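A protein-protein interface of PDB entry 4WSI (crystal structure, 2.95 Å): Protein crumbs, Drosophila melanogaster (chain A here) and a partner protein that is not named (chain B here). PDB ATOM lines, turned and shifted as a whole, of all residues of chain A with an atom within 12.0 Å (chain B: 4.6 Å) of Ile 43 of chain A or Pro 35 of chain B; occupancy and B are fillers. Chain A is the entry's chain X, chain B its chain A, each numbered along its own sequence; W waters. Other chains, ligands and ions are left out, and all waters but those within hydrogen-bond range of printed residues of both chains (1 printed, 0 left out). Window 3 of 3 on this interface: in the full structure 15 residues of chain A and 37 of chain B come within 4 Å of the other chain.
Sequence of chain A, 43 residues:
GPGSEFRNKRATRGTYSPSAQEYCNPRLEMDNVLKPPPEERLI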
ATOM      1  N   GLU A  39       9.260  -3.547  28.390  1.00  0.00           N
ATOM      2  CA  GLU A  39       9.309  -2.811  27.132  1.00  0.00           C
ATOM      3  C   GLU A  39       8.159  -1.816  27.073  1.00  0.00           C
ATOM      4  O   GLU A  39       7.079  -2.068  27.606  1.00  0.00           O
ATOM      5  CB  GLU A  39       9.256  -3.752  25.924  1.00  0.00           C
ATOM      6  CG  GLU A  39       7.887  -4.365  25.655  1.00  0.00           C
ATOM      7  CD  GLU A  39       7.728  -4.855  24.225  1.00  0.00           C
ATOM      8  OE1 GLU A  39       6.697  -5.499  23.928  1.00  0.00           O
ATOM      9  OE2 GLU A  39       8.625  -4.591  23.397  1.00  0.00           O
ATOM     10  N   GLU A  40       8.401  -0.677  26.440  1.00  0.00           N
ATOM     11  CA  GLU A  40       7.366   0.330  26.286  1.00  0.00           C
ATOM     12  C   GLU A  40       6.734   0.194  24.915  1.00  0.00           C
ATOM     13  O   GLU A  40       7.281  -0.455  24.025  1.00  0.00           O
ATOM     14  CB  GLU A  40       7.943   1.734  26.460  1.00  0.00           C
ATOM     15  CG  GLU A  40       8.590   1.977  27.810  1.00  0.00           C
ATOM     16  CD  GLU A  40       9.220   3.352  27.910  1.00  0.00           C
ATOM     17  OE1 GLU A  40       8.946   4.196  27.033  1.00  0.00           O
ATOM     18  OE2 GLU A  40       9.992   3.587  28.862  1.00  0.00           O
ATOM     19  N   ARG A  41       5.571   0.810  24.752  1.00  0.00           N
ATOM     20  CA  ARG A  41       4.868   0.762  23.486  1.00  0.00           C
ATOM     21  C   ARG A  41       4.100   2.064  23.280  1.00  0.00           C
ATOM     22  O   ARG A  41       3.498   2.595  24.212  1.00  0.00           O
ATOM     23  CB  ARG A  41       3.932  -0.442  23.455  1.00  0.00           C
ATOM     24  CG  ARG A  41       3.524  -0.852  22.064  1.00  0.00           C
ATOM     25  CD  ARG A  41       4.477  -1.855  21.444  1.00  0.00           C
ATOM     26  NE  ARG A  41       3.981  -2.295  20.143  1.00  0.00           N
ATOM     27  CZ  ARG A  41       4.455  -3.340  19.474  1.00  0.00           C
ATOM     28  NH1 ARG A  41       5.443  -4.065  19.982  1.00  0.00           N
ATOM     29  NH2 ARG A  41       3.935  -3.662  18.297  1.00  0.00           N
ATOM     30  N   LEU A  42       4.130   2.579  22.056  1.00  0.00           N
ATOM     31  CA  LEU A  42       3.597   3.908  21.767  1.00  0.00           C
ATOM     32  C   LEU A  42       2.089   3.911  21.525  1.00  0.00           C
ATOM     33  O   LEU A  42       1.592   3.198  20.660  1.00  0.00           O
ATOM     34  CB  LEU A  42       4.313   4.507  20.554  1.00  0.00           C
ATOM     35  CG  LEU A  42       3.989   5.963  20.215  1.00  0.00           C
ATOM     36  CD1 LEU A  42       4.536   6.905  21.278  1.00  0.00           C
ATOM     37  CD2 LEU A  42       4.527   6.323  18.839  1.00  0.00           C
ATOM     38  N   ILE A  43       1.362   4.725  22.283  1.00  0.00           N
ATOM     39  CA  ILE A  43      -0.072   4.869  22.056  1.00  0.00           C
ATOM     40  C   ILE A  43      -0.404   6.200  21.374  1.00  0.00           C
ATOM     41  O   ILE A  43      -1.353   6.295  20.591  1.00  0.00           O
ATOM     42  CB  ILE A  43      -0.889   4.711  23.357  1.00  0.00           C
ATOM     43  CG1 ILE A  43      -0.664   5.896  24.296  1.00  0.00           C
ATOM     44  CG2 ILE A  43      -0.547   3.400  24.046  1.00  0.00           C
ATOM     45  CD1 ILE A  43      -1.457   5.807  25.582  1.00  0.00           C
ATOM     46  OXT ILE A  43       0.273   7.212  21.574  1.00  0.00           O
ATOM     47  N   LYS B  30      -7.718  12.791  20.187  1.00  0.00           N
ATOM     48  CA  LYS B  30      -6.883  11.850  19.454  1.00  0.00           C
ATOM     49  C   LYS B  30      -7.248  11.902  17.975  1.00  0.00           C
ATOM     50  O   LYS B  30      -8.423  11.869  17.616  1.00  0.00           O
ATOM     51  CB  LYS B  30      -7.097  10.436  20.004  1.00  0.00           C
ATOM     52  CG  LYS B  30      -5.890   9.515  19.920  1.00  0.00           C
ATOM     53  CD  LYS B  30      -5.834   8.766  18.604  1.00  0.00           C
ATOM     54  CE  LYS B  30      -4.714   7.738  18.611  1.00  0.00           C
ATOM     55  NZ  LYS B  30      -4.519   7.113  17.273  1.00  0.00           N
ATOM     56  N   ASP B  33      -5.157   7.584  13.288  1.00  0.00           N
ATOM     57  CA  ASP B  33      -3.835   7.126  12.862  1.00  0.00           C
ATOM     58  C   ASP B  33      -2.686   8.043  13.295  1.00  0.00           C
ATOM     59  O   ASP B  33      -1.578   7.953  12.767  1.00  0.00           O
ATOM     60  CB  ASP B  33      -3.804   6.862  11.354  1.00  0.00           C
ATOM     61  CG  ASP B  33      -4.849   5.850  10.921  1.00  0.00           C
ATOM     62  OD1 ASP B  33      -5.043   4.849  11.643  1.00  0.00           O
ATOM     63  OD2 ASP B  33      -5.483   6.060   9.865  1.00  0.00           O
ATOM     64  N   ILE B  34      -2.953   8.914  14.264  1.00  0.00           N
ATOM     65  CA  ILE B  34      -1.918   9.780  14.826  1.00  0.00           C
ATOM     66  C   ILE B  34      -1.775   9.564  16.332  1.00  0.00           C
ATOM     67  O   ILE B  34      -2.640   9.980  17.107  1.00  0.00           O
ATOM     68  CB  ILE B  34      -2.219  11.273  14.573  1.00  0.00           C
ATOM     69  CG1 ILE B  34      -2.390  11.550  13.075  1.00  0.00           C
ATOM     70  CG2 ILE B  34      -1.116  12.139  15.157  1.00  0.00           C
ATOM     71  CD1 ILE B  34      -1.163  11.245  12.249  1.00  0.00           C
ATOM     72  N   PRO B  35      -0.679   8.910  16.748  1.00  0.00           N
ATOM     73  CA  PRO B  35      -0.376   8.599  18.151  1.00  0.00           C
ATOM     74  C   PRO B  35      -0.366   9.828  19.060  1.00  0.00           C
ATOM     75  O   PRO B  35       0.036  10.911  18.640  1.00  0.00           O
ATOM     76  CB  PRO B  35       1.020   7.980  18.071  1.00  0.00           C
ATOM     77  CG  PRO B  35       1.063   7.357  16.724  1.00  0.00           C
ATOM     78  CD  PRO B  35       0.306   8.306  15.833  1.00  0.00           C
ATOM     79  N   LEU B  36      -0.812   9.644  20.300  1.00  0.00           N
ATOM     80  CA  LEU B  36      -0.876  10.726  21.277  1.00  0.00           C
ATOM     81  C   LEU B  36       0.508  11.238  21.666  1.00  0.00           C
ATOM     82  O   LEU B  36       0.671  12.408  22.015  1.00  0.00           O
ATOM     83  CB  LEU B  36      -1.619  10.264  22.531  1.00  0.00           C
ATOM     84  CG  LEU B  36      -3.135  10.126  22.415  1.00  0.00           C
ATOM     85  CD1 LEU B  36      -3.719   9.572  23.703  1.00  0.00           C
ATOM     86  CD2 LEU B  36      -3.754  11.472  22.080  1.00  0.00           C
ATOM     87  N   GLY B  37       1.498  10.355  21.607  1.00  0.00           N
ATOM     88  CA  GLY B  37       2.847  10.702  22.007  1.00  0.00           C
ATOM     89  C   GLY B  37       3.143  10.315  23.443  1.00  0.00           C
ATOM     90  O   GLY B  37       3.894  10.998  24.138  1.00  0.00           O
ATOM     91  N   ALA B  38       2.543   9.219  23.894  1.00  0.00           N
ATOM     92  CA  ALA B  38       2.815   8.691  25.225  1.00  0.00           C
ATOM     93  C   ALA B  38       3.065   7.197  25.124  1.00  0.00           C
ATOM     94  O   ALA B  38       2.433   6.516  24.322  1.00  0.00           O
ATOM     95  CB  ALA B  38       1.655   8.970  26.153  1.00  0.00           C
ATOM     96  N   VAL B  40       3.424   3.321  27.110  1.00  0.00           N
ATOM     97  CA  VAL B  40       2.946   2.570  28.259  1.00  0.00           C
ATOM     98  C   VAL B  40       3.740   1.289  28.456  1.00  0.00           C
ATOM     99  O   VAL B  40       4.097   0.609  27.492  1.00  0.00           O
ATOM    100  CB  VAL B  40       1.453   2.225  28.130  1.00  0.00           C
ATOM    101  CG1 VAL B  40       0.611   3.486  28.233  1.00  0.00           C
ATOM    102  CG2 VAL B  40       1.186   1.501  26.814  1.00  0.00           C
ATOM    103  N   ILE B  49       1.586   4.712  32.296  1.00  0.00           N
ATOM    104  CA  ILE B  49       2.164   5.731  31.428  1.00  0.00           C
ATOM    105  C   ILE B  49       3.622   5.905  31.827  1.00  0.00           C
ATOM    106  O   ILE B  49       3.913   6.431  32.901  1.00  0.00           O
ATOM    107  CB  ILE B  49       1.452   7.082  31.595  1.00  0.00           C
ATOM    108  CG1 ILE B  49      -0.031   6.955  31.251  1.00  0.00           C
ATOM    109  CG2 ILE B  49       2.108   8.137  30.725  1.00  0.00           C
ATOM    110  CD1 ILE B  49      -0.297   6.653  29.795  1.00  0.00           C
ATOM    111  N   VAL B  86      -2.958  -2.799  24.258  1.00  0.00           N
ATOM    112  CA  VAL B  86      -3.220  -1.373  24.417  1.00  0.00           C
ATOM    113  C   VAL B  86      -2.718  -0.611  23.193  1.00  0.00           C
ATOM    114  O   VAL B  86      -3.336   0.358  22.750  1.00  0.00           O
ATOM    115  CB  VAL B  86      -2.550  -0.815  25.686  1.00  0.00           C
ATOM    116  CG1 VAL B  86      -2.915   0.644  25.884  1.00  0.00           C
ATOM    117  CG2 VAL B  86      -2.957  -1.637  26.899  1.00  0.00           C
ATOM    118  N   LEU B  90      -5.478   1.604  20.866  1.00  0.00           N
ATOM    119  CA  LEU B  90      -5.434   3.046  20.638  1.00  0.00           C
ATOM    120  C   LEU B  90      -5.074   3.422  19.201  1.00  0.00           C
ATOM    121  O   LEU B  90      -5.364   4.531  18.754  1.00  0.00           O
ATOM    122  CB  LEU B  90      -4.493   3.741  21.625  1.00  0.00           C
ATOM    123  CG  LEU B  90      -5.150   4.101  22.956  1.00  0.00           C
ATOM    124  CD1 LEU B  90      -5.073   2.937  23.926  1.00  0.00           C
ATOM    125  CD2 LEU B  90      -4.529   5.349  23.544  1.00  0.00           C
ATOM    126  N   LEU B 172       6.736  13.683  16.267  1.00  0.00           N
ATOM    127  CA  LEU B 172       7.205  13.259  17.579  1.00  0.00           C
ATOM    128  C   LEU B 172       8.722  13.229  17.634  1.00  0.00           C
ATOM    129  O   LEU B 172       9.386  12.943  16.638  1.00  0.00           O
ATOM    130  CB  LEU B 172       6.685  11.860  17.904  1.00  0.00           C
ATOM    131  CG  LEU B 172       5.196  11.665  18.180  1.00  0.00           C
ATOM    132  CD1 LEU B 172       4.929  10.209  18.508  1.00  0.00           C
ATOM    133  CD2 LEU B 172       4.737  12.570  19.312  1.00  0.00           C
HETATM  134  O   HOH W   1      -2.362   5.763  17.414  1.00  0.00           O
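The backbone NH (N) of Leu 36 of chain B lies within hydrogen-bond range of the chain-end carboxylate (OXT) of Ile 43 of chain A, 3.0 Å away.
O of Ala 38 of chain B is in hydrogen-bond range of N of Ile 43 of chain A, 2.9 Å away.
N of Val 40 of chain B sits at hydrogen-bond distance from O of Arg 41 of chain A (3.0 Å).
The chain-end carboxylate of Ile 43 of chain A sits at hydrogen-bond distance from the backbone NH of Gly 37 of chain B.
Water W1 bridges NZ of Lys 30 of chain B (2.5 Å) and O of Ile 43 of chain A (3.4 Å).
Among the printed residues, pairs that only touch across the chains: Glu 40 of chain A with Val 40 of chain B, Leu 42 of chain A with Pro 35 of chain B, Leu 42 of chain A with Ala 38 of chain B, Leu 42 of chain A with Leu 172 of chain B, Ile 43 of chain A with Pro 35 of chain B, Ile 43 of chain A with Val 40 of chain B and Ile 43 of chain A with Leu 90 of chain B.
Hydrophobic or aromatic side chains of chain A within 4 Å of the printed part of chain B: Leu 42 and Ile 43.
Of the 12 printed residues of chain B, 7 touch a printed residue of chain A.
Hydrophobic or aromatic side chains of chain B within 4 Å of the printed part of chain A: Pro 35, Leu 36, Val 40, Leu 90 and Leu 172.
Among the printed residues, no Asp or Glu carboxylate lies within 4 Å of a Lys or Arg side-chain nitrogen of the other chain.
NZ of Lys 30 of chain B is in hydrogen-bond range of O of Leu 90 of chain B.
Of the printed residues of chain B, Glu 40 of chain A touches Val 40.
Printed residues of chain B within 4 Å of Ile 43 of chain A: Pro 35 (3.5 Å), Leu 36 (3.0 Å), Gly 37 (3.4 Å), Ala 38 (2.9 Å), Val 40 (3.8 Å) and Leu 90 (3.7 Å).
Lys 30 of chain B touches none of the printed residues of chain A.
Of chain A, only Leu 42 (3.95 Å) and Ile 43 (3.5 Å) come within 4 Å of Pro 35 of chain B.
Of the printed residues of chain A, Leu 36 of chain B touches Ile 43.
Of chain A, only Ile 43 comes within 4 Å of Gly 37 of chain B.
Of the printed residues of chain A, Val 40 of chain B touches Glu 40, Arg 41 and Ile 43.
Ile 49 of chain B touches none of the printed residues of chain A.
No residue of chain A comes within 4 Å of Val 86 of chain B.
The nearest residue of chain B that does not touch Ile 43 of chain A is Val 86 of chain B (4.1 Å).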
